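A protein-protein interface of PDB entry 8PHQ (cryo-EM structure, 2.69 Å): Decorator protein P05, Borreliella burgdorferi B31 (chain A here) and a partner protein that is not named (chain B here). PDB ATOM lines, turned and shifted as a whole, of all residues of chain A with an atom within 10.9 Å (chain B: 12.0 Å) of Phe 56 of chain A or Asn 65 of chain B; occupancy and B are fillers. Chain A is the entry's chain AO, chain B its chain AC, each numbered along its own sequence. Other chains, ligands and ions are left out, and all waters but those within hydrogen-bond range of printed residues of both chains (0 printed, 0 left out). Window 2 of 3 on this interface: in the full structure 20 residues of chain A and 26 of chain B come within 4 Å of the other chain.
The side-chain hydroxyl (OG) of Ser 68 of chain B sits at hydrogen-bond distance from the backbone carbonyl oxygen (O) of Asn 56 of chain B.
The side-chain hydroxyl (OG1) of Thr 58 of chain B lies within hydrogen-bond range of the backbone NH (N) of Ser 68 of chain B (2.9 Å).
The backbone NH (N) of Phe 56 of chain A sits close to the side-chain hydroxyl (OG) of Ser 54 of chain A (3.2 Å).
The side-chain amide oxygen (OD1) of Asn 65 of chain B lies within hydrogen-bond range of the side-chain hydroxyl (OG) of Ser 54 of chain A, at 3.1 Å.
The backbone NH of Thr 53 of chain A is in hydrogen-bond range of the backbone carbonyl oxygen of Ile 67 of chain B, 3.3 Å away.
The backbone carbonyl oxygen (O) of Thr 51 of chain A lies within hydrogen-bond range of the side-chain hydroxyl (OG1) of Thr 69 of chain B (2.9 Å).
CA of Ser 68 of chain B touches O of Thr 51 of chain A, at 3.6 Å.
Arg 52 of chain A touches Thr 66 of chain B.
CA of Arg 52 of chain A touches O of Ile 67 of chain B (3.5 Å).
Arg 52 of chain A touches Ser 68 of chain B (CG to OG, 3.4 Å).
Asn 65 of chain B touches Thr 53 of chain A (O to O, 3.8 Å).
Thr 66 of chain B touches Ser 54 of chain A (OG1 to CB, 3.6 Å).
Lys 55 of chain A touches Asn 65 of chain B (N to O, 3.8 Å).
Phe 56 of chain A touches Asn 65 of chain B.
Phe 56 of chain A touches one residue of chain B.
Of chain A, only Thr 53 (3.8 Å), Ser 54 (3.1 Å), Lys 55 (3.8 Å) and Phe 56 (3.8 Å) come within 4 Å of Asn 65 of chain B.
No residue of chain B comes within 4 Å of Asp 57 of chain A.
No residue of chain A comes within 4 Å of Val 64 of chain B.
Ile 67 of chain B touches just these residues of chain A: Arg 52 and Thr 53.
Printed residues of chain A within 4 Å of Ser 68 of chain B: Thr 51 (3.6 Å) and Arg 52 (3.4 Å).
Printed residues of chain B within 4 Å of Thr 51 of chain A: Ser 68 and Thr 69.
Of the printed residues of chain A, Thr 66 of chain B touches Arg 52 (3.9 Å) and Ser 54 (3.6 Å).
Of the printed residues of chain B, Thr 53 of chain A touches Asn 65 and Ile 67.
Of the printed residues of chain A, Thr 69 of chain B touches Thr 51 (2.9 Å).
The nearest residue of chain A that does not touch Asn 65 of chain B is Asp 57 of chain A (6.9 Å).
The nearest printed residue of chain A that does not touch Thr 66 of chain B is Thr 53 of chain A (4.01 Å).
Of the 14 printed residues of chain B, 5 touch a printed residue of chain A.
Printed residues of chain B that touch a printed residue of chain A: Asn 65, Thr 66, Ile 67, Ser 68 and Thr 69.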
ATOM      1  N   THR A  51     -24.289  25.237  -0.170  1.00  0.00           N
ATOM      2  CA  THR A  51     -25.473  24.635  -0.772  1.00  0.00           C
ATOM      3  C   THR A  51     -25.199  23.205  -1.221  1.00  0.00           C
ATOM      4  O   THR A  51     -26.022  22.310  -1.002  1.00  0.00           O
ATOM      5  CB  THR A  51     -25.957  25.483  -1.948  1.00  0.00           C
ATOM      6  OG1 THR A  51     -24.992  25.431  -3.006  1.00  0.00           O
ATOM      7  CG2 THR A  51     -26.146  26.925  -1.517  1.00  0.00           C
ATOM      8  N   ARG A  52     -24.050  22.972  -1.850  1.00  0.00           N
ATOM      9  CA  ARG A  52     -23.590  21.635  -2.204  1.00  0.00           C
ATOM     10  C   ARG A  52     -22.212  21.429  -1.598  1.00  0.00           C
ATOM     11  O   ARG A  52     -21.297  22.220  -1.853  1.00  0.00           O
ATOM     12  CB  ARG A  52     -23.547  21.442  -3.719  1.00  0.00           C
ATOM     13  CG  ARG A  52     -24.881  21.629  -4.405  1.00  0.00           C
ATOM     14  CD  ARG A  52     -24.695  21.811  -5.895  1.00  0.00           C
ATOM     15  NE  ARG A  52     -23.736  20.856  -6.435  1.00  0.00           N
ATOM     16  CZ  ARG A  52     -23.305  20.858  -7.687  1.00  0.00           C
ATOM     17  NH1 ARG A  52     -23.732  21.754  -8.561  1.00  0.00           N
ATOM     18  NH2 ARG A  52     -22.426  19.938  -8.074  1.00  0.00           N
ATOM     19  N   THR A  53     -22.063  20.372  -0.809  1.00  0.00           N
ATOM     20  CA  THR A  53     -20.835  20.102  -0.078  1.00  0.00           C
ATOM     21  C   THR A  53     -20.326  18.707  -0.413  1.00  0.00           C
ATOM     22  O   THR A  53     -21.103  17.751  -0.476  1.00  0.00           O
ATOM     23  CB  THR A  53     -21.059  20.231   1.433  1.00  0.00           C
ATOM     24  OG1 THR A  53     -21.549  21.542   1.736  1.00  0.00           O
ATOM     25  CG2 THR A  53     -19.764  19.995   2.195  1.00  0.00           C
ATOM     26  N   SER A  54     -19.020  18.600  -0.625  1.00  0.00           N
ATOM     27  CA  SER A  54     -18.364  17.325  -0.859  1.00  0.00           C
ATOM     28  C   SER A  54     -17.732  16.814   0.429  1.00  0.00           C
ATOM     29  O   SER A  54     -17.298  17.592   1.281  1.00  0.00           O
ATOM     30  CB  SER A  54     -17.295  17.451  -1.944  1.00  0.00           C
ATOM     31  OG  SER A  54     -16.507  16.277  -2.015  1.00  0.00           O
ATOM     32  N   LYS A  55     -17.688  15.487   0.563  1.00  0.00           N
ATOM     33  CA  LYS A  55     -17.047  14.881   1.723  1.00  0.00           C
ATOM     34  C   LYS A  55     -15.557  15.191   1.773  1.00  0.00           C
ATOM     35  O   LYS A  55     -14.971  15.210   2.860  1.00  0.00           O
ATOM     36  CB  LYS A  55     -17.281  13.367   1.711  1.00  0.00           C
ATOM     37  CG  LYS A  55     -16.509  12.592   2.766  1.00  0.00           C
ATOM     38  CD  LYS A  55     -16.725  11.096   2.632  1.00  0.00           C
ATOM     39  CE  LYS A  55     -15.963  10.334   3.703  1.00  0.00           C
ATOM     40  NZ  LYS A  55     -16.284   8.881   3.688  1.00  0.00           N
ATOM     41  N   PHE A  56     -14.942  15.467   0.626  1.00  0.00           N
ATOM     42  CA  PHE A  56     -13.509  15.735   0.530  1.00  0.00           C
ATOM     43  C   PHE A  56     -13.206  17.224   0.450  1.00  0.00           C
ATOM     44  O   PHE A  56     -12.284  17.644  -0.252  1.00  0.00           O
ATOM     45  CB  PHE A  56     -12.923  14.994  -0.665  1.00  0.00           C
ATOM     46  CG  PHE A  56     -13.269  13.535  -0.689  1.00  0.00           C
ATOM     47  CD1 PHE A  56     -12.881  12.704   0.348  1.00  0.00           C
ATOM     48  CD2 PHE A  56     -13.999  12.999  -1.733  1.00  0.00           C
ATOM     49  CE1 PHE A  56     -13.203  11.364   0.337  1.00  0.00           C
ATOM     50  CE2 PHE A  56     -14.325  11.658  -1.748  1.00  0.00           C
ATOM     51  CZ  PHE A  56     -13.927  10.840  -0.712  1.00  0.00           C
ATOM     52  N   ASP A  57     -13.977  18.045   1.158  1.00  0.00           N
ATOM     53  CA  ASP A  57     -13.691  19.467   1.279  1.00  0.00           C
ATOM     54  C   ASP A  57     -12.864  19.713   2.534  1.00  0.00           C
ATOM     55  O   ASP A  57     -13.234  19.268   3.625  1.00  0.00           O
ATOM     56  CB  ASP A  57     -14.986  20.279   1.328  1.00  0.00           C
ATOM     57  CG  ASP A  57     -15.529  20.594  -0.052  1.00  0.00           C
ATOM     58  OD1 ASP A  57     -14.852  20.267  -1.049  1.00  0.00           O
ATOM     59  OD2 ASP A  57     -16.637  21.165  -0.140  1.00  0.00           O
ATOM     60  N   LYS A  58     -11.748  20.417   2.375  1.00  0.00           N
ATOM     61  CA  LYS A  58     -10.848  20.684   3.488  1.00  0.00           C
ATOM     62  C   LYS A  58     -11.379  21.837   4.331  1.00  0.00           C
ATOM     63  O   LYS A  58     -11.681  22.913   3.807  1.00  0.00           O
ATOM     64  CB  LYS A  58      -9.447  21.002   2.968  1.00  0.00           C
ATOM     65  CG  LYS A  58      -8.411  21.207   4.056  1.00  0.00           C
ATOM     66  CD  LYS A  58      -7.008  21.185   3.479  1.00  0.00           C
ATOM     67  CE  LYS A  58      -5.963  21.379   4.562  1.00  0.00           C
ATOM     68  NZ  LYS A  58      -4.581  21.255   4.030  1.00  0.00           N
ATOM     69  N   LEU A  59     -11.492  21.609   5.636  1.00  0.00           N
ATOM     70  CA  LEU A  59     -12.019  22.591   6.574  1.00  0.00           C
ATOM     71  C   LEU A  59     -10.981  22.860   7.654  1.00  0.00           C
ATOM     72  O   LEU A  59     -10.490  21.922   8.290  1.00  0.00           O
ATOM     73  CB  LEU A  59     -13.322  22.097   7.205  1.00  0.00           C
ATOM     74  CG  LEU A  59     -14.419  21.677   6.229  1.00  0.00           C
ATOM     75  CD1 LEU A  59     -15.656  21.224   6.980  1.00  0.00           C
ATOM     76  CD2 LEU A  59     -14.749  22.813   5.278  1.00  0.00           C
ATOM     77  N   GLU A  60     -10.655  24.134   7.866  1.00  0.00           N
ATOM     78  CA  GLU A  60      -9.642  24.539   8.832  1.00  0.00           C
ATOM     79  C   GLU A  60     -10.274  25.472   9.853  1.00  0.00           C
ATOM     80  O   GLU A  60     -10.954  26.427   9.478  1.00  0.00           O
ATOM     81  CB  GLU A  60      -8.484  25.243   8.126  1.00  0.00           C
ATOM     82  CG  GLU A  60      -7.621  24.328   7.285  1.00  0.00           C
ATOM     83  CD  GLU A  60      -6.401  25.032   6.734  1.00  0.00           C
ATOM     84  OE1 GLU A  60      -6.295  26.263   6.912  1.00  0.00           O
ATOM     85  OE2 GLU A  60      -5.551  24.357   6.118  1.00  0.00           O
ATOM     86  N   ILE A 115     -13.072  27.632   8.071  1.00  0.00           N
ATOM     87  CA  ILE A 115     -12.606  28.295   6.864  1.00  0.00           C
ATOM     88  C   ILE A 115     -12.356  27.244   5.796  1.00  0.00           C
ATOM     89  O   ILE A 115     -11.767  26.193   6.074  1.00  0.00           O
ATOM     90  CB  ILE A 115     -11.330  29.113   7.132  1.00  0.00           C
ATOM     91  CG1 ILE A 115     -11.611  30.215   8.148  1.00  0.00           C
ATOM     92  CG2 ILE A 115     -10.777  29.693   5.844  1.00  0.00           C
ATOM     93  CD1 ILE A 115     -10.404  31.034   8.479  1.00  0.00           C
ATOM     94  N   VAL A 116     -12.821  27.524   4.586  1.00  0.00           N
ATOM     95  CA  VAL A 116     -12.480  26.750   3.399  1.00  0.00           C
ATOM     96  C   VAL A 116     -11.304  27.447   2.726  1.00  0.00           C
ATOM     97  O   VAL A 116     -11.448  28.605   2.309  1.00  0.00           O
ATOM     98  CB  VAL A 116     -13.674  26.632   2.440  1.00  0.00           C
ATOM     99  CG1 VAL A 116     -13.292  25.830   1.211  1.00  0.00           C
ATOM    100  CG2 VAL A 116     -14.863  26.010   3.147  1.00  0.00           C
ATOM    101  N   PRO A 117     -10.140  26.808   2.619  1.00  0.00           N
ATOM    102  CA  PRO A 117      -8.991  27.475   2.001  1.00  0.00           C
ATOM    103  C   PRO A 117      -9.279  27.845   0.554  1.00  0.00           C
ATOM    104  O   PRO A 117     -10.082  27.205  -0.127  1.00  0.00           O
ATOM    105  CB  PRO A 117      -7.876  26.429   2.099  1.00  0.00           C
ATOM    106  CG  PRO A 117      -8.279  25.556   3.230  1.00  0.00           C
ATOM    107  CD  PRO A 117      -9.776  25.506   3.200  1.00  0.00           C
ATOM    108  N   THR A 119      -7.639  27.379  -1.953  1.00  0.00           N
ATOM    109  CA  THR A 119      -7.276  26.310  -2.875  1.00  0.00           C
ATOM    110  C   THR A 119      -8.397  25.301  -3.078  1.00  0.00           C
ATOM    111  O   THR A 119      -8.252  24.397  -3.906  1.00  0.00           O
ATOM    112  CB  THR A 119      -6.022  25.588  -2.376  1.00  0.00           C
ATOM    113  OG1 THR A 119      -6.245  25.104  -1.046  1.00  0.00           O
ATOM    114  CG2 THR A 119      -4.833  26.529  -2.373  1.00  0.00           C
ATOM    115  N   ASN A 120      -9.498  25.428  -2.345  1.00  0.00           N
ATOM    116  CA  ASN A 120     -10.644  24.542  -2.464  1.00  0.00           C
ATOM    117  C   ASN A 120     -11.855  25.350  -2.910  1.00  0.00           C
ATOM    118  O   ASN A 120     -12.123  26.427  -2.371  1.00  0.00           O
ATOM    119  CB  ASN A 120     -10.926  23.841  -1.131  1.00  0.00           C
ATOM    120  CG  ASN A 120     -11.970  22.753  -1.250  1.00  0.00           C
ATOM    121  OD1 ASN A 120     -12.525  22.518  -2.322  1.00  0.00           O
ATOM    122  ND2 ASN A 120     -12.240  22.076  -0.143  1.00  0.00           N
ATOM    123  N   ASN A 121     -12.581  24.829  -3.895  1.00  0.00           N
ATOM    124  CA  ASN A 121     -13.720  25.545  -4.447  1.00  0.00           C
ATOM    125  C   ASN A 121     -14.915  25.473  -3.500  1.00  0.00           C
ATOM    126  O   ASN A 121     -14.992  24.618  -2.615  1.00  0.00           O
ATOM    127  CB  ASN A 121     -14.097  24.988  -5.820  1.00  0.00           C
ATOM    128  CG  ASN A 121     -14.737  23.620  -5.736  1.00  0.00           C
ATOM    129  OD1 ASN A 121     -14.135  22.671  -5.239  1.00  0.00           O
ATOM    130  ND2 ASN A 121     -15.965  23.511  -6.229  1.00  0.00           N
ATOM    131  N   PHE A 122     -15.856  26.393  -3.700  1.00  0.00           N
ATOM    132  CA  PHE A 122     -16.980  26.550  -2.788  1.00  0.00           C
ATOM    133  C   PHE A 122     -18.188  27.070  -3.551  1.00  0.00           C
ATOM    134  O   PHE A 122     -18.044  27.839  -4.502  1.00  0.00           O
ATOM    135  CB  PHE A 122     -16.623  27.507  -1.644  1.00  0.00           C
ATOM    136  CG  PHE A 122     -17.779  27.846  -0.749  1.00  0.00           C
ATOM    137  CD1 PHE A 122     -18.314  26.897   0.101  1.00  0.00           C
ATOM    138  CD2 PHE A 122     -18.330  29.115  -0.760  1.00  0.00           C
ATOM    139  CE1 PHE A 122     -19.376  27.207   0.927  1.00  0.00           C
ATOM    140  CE2 PHE A 122     -19.393  29.430   0.062  1.00  0.00           C
ATOM    141  CZ  PHE A 122     -19.917  28.475   0.905  1.00  0.00           C
ATOM    142  N   ASN B  56     -31.586  22.303  -5.589  1.00  0.00           N
ATOM    143  CA  ASN B  56     -32.251  21.199  -6.254  1.00  0.00           C
ATOM    144  C   ASN B  56     -31.554  19.887  -5.895  1.00  0.00           C
ATOM    145  O   ASN B  56     -30.357  19.876  -5.600  1.00  0.00           O
ATOM    146  CB  ASN B  56     -32.237  21.392  -7.768  1.00  0.00           C
ATOM    147  CG  ASN B  56     -33.078  22.567  -8.214  1.00  0.00           C
ATOM    148  OD1 ASN B  56     -34.272  22.637  -7.928  1.00  0.00           O
ATOM    149  ND2 ASN B  56     -32.461  23.493  -8.938  1.00  0.00           N
ATOM    150  N   PRO B  57     -32.278  18.770  -5.909  1.00  0.00           N
ATOM    151  CA  PRO B  57     -31.649  17.487  -5.584  1.00  0.00           C
ATOM    152  C   PRO B  57     -30.584  17.119  -6.604  1.00  0.00           C
ATOM    153  O   PRO B  57     -30.525  17.661  -7.708  1.00  0.00           O
ATOM    154  CB  PRO B  57     -32.820  16.498  -5.610  1.00  0.00           C
ATOM    155  CG  PRO B  57     -33.846  17.151  -6.463  1.00  0.00           C
ATOM    156  CD  PRO B  57     -33.712  18.619  -6.211  1.00  0.00           C
ATOM    157  N   THR B  58     -29.714  16.196  -6.208  1.00  0.00           N
ATOM    158  CA  THR B  58     -28.583  15.780  -7.025  1.00  0.00           C
ATOM    159  C   THR B  58     -28.933  14.507  -7.782  1.00  0.00           C
ATOM    160  O   THR B  58     -29.470  13.560  -7.198  1.00  0.00           O
ATOM    161  CB  THR B  58     -27.343  15.556  -6.158  1.00  0.00           C
ATOM    162  OG1 THR B  58     -26.929  16.801  -5.584  1.00  0.00           O
ATOM    163  CG2 THR B  58     -26.203  14.992  -6.987  1.00  0.00           C
ATOM    164  N   THR B  59     -28.635  14.490  -9.079  1.00  0.00           N
ATOM    165  CA  THR B  59     -28.832  13.300  -9.898  1.00  0.00           C
ATOM    166  C   THR B  59     -27.669  12.339  -9.682  1.00  0.00           C
ATOM    167  O   THR B  59     -26.510  12.699  -9.912  1.00  0.00           O
ATOM    168  CB  THR B  59     -28.945  13.675 -11.373  1.00  0.00           C
ATOM    169  OG1 THR B  59     -30.084  14.521 -11.569  1.00  0.00           O
ATOM    170  CG2 THR B  59     -29.093  12.430 -12.228  1.00  0.00           C
ATOM    171  N   ILE B  60     -27.975  11.120  -9.249  1.00  0.00           N
ATOM    172  CA  ILE B  60     -26.956  10.117  -8.960  1.00  0.00           C
ATOM    173  C   ILE B  60     -26.707   9.325 -10.238  1.00  0.00           C
ATOM    174  O   ILE B  60     -27.464   8.419 -10.585  1.00  0.00           O
ATOM    175  CB  ILE B  60     -27.364   9.210  -7.800  1.00  0.00           C
ATOM    176  CG1 ILE B  60     -27.717  10.054  -6.577  1.00  0.00           C
ATOM    177  CG2 ILE B  60     -26.249   8.234  -7.472  1.00  0.00           C
ATOM    178  CD1 ILE B  60     -26.606  10.987  -6.154  1.00  0.00           C
ATOM    179  N   ALA B  61     -25.632   9.671 -10.939  1.00  0.00           N
ATOM    180  CA  ALA B  61     -25.225   8.979 -12.153  1.00  0.00           C
ATOM    181  C   ALA B  61     -23.706   8.971 -12.217  1.00  0.00           C
ATOM    182  O   ALA B  61     -23.074  10.010 -12.008  1.00  0.00           O
ATOM    183  CB  ALA B  61     -25.807   9.654 -13.398  1.00  0.00           C
ATOM    184  N   ASN B  62     -23.134   7.808 -12.507  1.00  0.00           N
ATOM    185  CA  ASN B  62     -21.674   7.613 -12.558  1.00  0.00           C
ATOM    186  C   ASN B  62     -21.105   7.999 -11.188  1.00  0.00           C
ATOM    187  O   ASN B  62     -21.687   7.636 -10.155  1.00  0.00           O
ATOM    188  CB  ASN B  62     -21.086   8.370 -13.730  1.00  0.00           C
ATOM    189  CG  ASN B  62     -21.450   7.754 -15.062  1.00  0.00           C
ATOM    190  OD1 ASN B  62     -22.121   6.725 -15.119  1.00  0.00           O
ATOM    191  ND2 ASN B  62     -21.007   8.382 -16.143  1.00  0.00           N
ATOM    192  N   GLU B  63     -19.993   8.725 -11.141  1.00  0.00           N
ATOM    193  CA  GLU B  63     -19.325   9.071  -9.895  1.00  0.00           C
ATOM    194  C   GLU B  63     -19.588  10.530  -9.554  1.00  0.00           C
ATOM    195  O   GLU B  63     -19.441  11.408 -10.410  1.00  0.00           O
ATOM    196  CB  GLU B  63     -17.821   8.825 -10.001  1.00  0.00           C
ATOM    197  CG  GLU B  63     -17.439   7.381 -10.252  1.00  0.00           C
ATOM    198  CD  GLU B  63     -15.942   7.193 -10.367  1.00  0.00           C
ATOM    199  OE1 GLU B  63     -15.225   7.539  -9.406  1.00  0.00           O
ATOM    200  OE2 GLU B  63     -15.480   6.702 -11.419  1.00  0.00           O
ATOM    201  N   VAL B  64     -19.981  10.783  -8.308  1.00  0.00           N
ATOM    202  CA  VAL B  64     -20.177  12.144  -7.821  1.00  0.00           C
ATOM    203  C   VAL B  64     -20.138  12.116  -6.299  1.00  0.00           C
ATOM    204  O   VAL B  64     -20.687  11.210  -5.667  1.00  0.00           O
ATOM    205  CB  VAL B  64     -21.495  12.753  -8.362  1.00  0.00           C
ATOM    206  CG1 VAL B  64     -22.706  11.989  -7.850  1.00  0.00           C
ATOM    207  CG2 VAL B  64     -21.593  14.221  -7.993  1.00  0.00           C
ATOM    208  N   ASN B  65     -19.457  13.104  -5.714  1.00  0.00           N
ATOM    209  CA  ASN B  65     -19.432  13.258  -4.269  1.00  0.00           C
ATOM    210  C   ASN B  65     -19.809  14.657  -3.802  1.00  0.00           C
ATOM    211  O   ASN B  65     -19.761  14.921  -2.596  1.00  0.00           O
ATOM    212  CB  ASN B  65     -18.051  12.887  -3.703  1.00  0.00           C
ATOM    213  CG  ASN B  65     -16.912  13.496  -4.489  1.00  0.00           C
ATOM    214  OD1 ASN B  65     -16.818  14.713  -4.631  1.00  0.00           O
ATOM    215  ND2 ASN B  65     -16.029  12.647  -4.999  1.00  0.00           N
ATOM    216  N   THR B  66     -20.181  15.556  -4.713  1.00  0.00           N
ATOM    217  CA  THR B  66     -20.679  16.883  -4.364  1.00  0.00           C
ATOM    218  C   THR B  66     -22.196  16.863  -4.499  1.00  0.00           C
ATOM    219  O   THR B  66     -22.727  16.853  -5.613  1.00  0.00           O
ATOM    220  CB  THR B  66     -20.060  17.954  -5.257  1.00  0.00           C
ATOM    221  OG1 THR B  66     -18.641  17.765  -5.313  1.00  0.00           O
ATOM    222  CG2 THR B  66     -20.356  19.337  -4.708  1.00  0.00           C
ATOM    223  N   ILE B  67     -22.892  16.858  -3.365  1.00  0.00           N
ATOM    224  CA  ILE B  67     -24.324  16.598  -3.317  1.00  0.00           C
ATOM    225  C   ILE B  67     -25.018  17.730  -2.573  1.00  0.00           C
ATOM    226  O   ILE B  67     -24.487  18.258  -1.591  1.00  0.00           O
ATOM    227  CB  ILE B  67     -24.613  15.238  -2.651  1.00  0.00           C
ATOM    228  CG1 ILE B  67     -23.792  14.147  -3.339  1.00  0.00           C
ATOM    229  CG2 ILE B  67     -26.093  14.911  -2.693  1.00  0.00           C
ATOM    230  CD1 ILE B  67     -23.950  12.798  -2.736  1.00  0.00           C
ATOM    231  N   SER B  68     -26.204  18.102  -3.050  1.00  0.00           N
ATOM    232  CA  SER B  68     -26.968  19.177  -2.435  1.00  0.00           C
ATOM    233  C   SER B  68     -27.365  18.808  -1.011  1.00  0.00           C
ATOM    234  O   SER B  68     -27.578  17.639  -0.683  1.00  0.00           O
ATOM    235  CB  SER B  68     -28.214  19.483  -3.264  1.00  0.00           C
ATOM    236  OG  SER B  68     -27.861  19.991  -4.538  1.00  0.00           O
ATOM    237  N   THR B  69     -27.474  19.825  -0.163  1.00  0.00           N
ATOM    238  CA  THR B  69     -27.652  19.637   1.268  1.00  0.00           C
ATOM    239  C   THR B  69     -29.020  20.124   1.727  1.00  0.00           C
ATOM    240  O   THR B  69     -29.635  20.992   1.104  1.00  0.00           O
ATOM    241  CB  THR B  69     -26.564  20.371   2.055  1.00  0.00           C
ATOM    242  OG1 THR B  69     -26.631  21.773   1.769  1.00  0.00           O
ATOM    243  CG2 THR B  69     -25.187  19.850   1.679  1.00  0.00           C
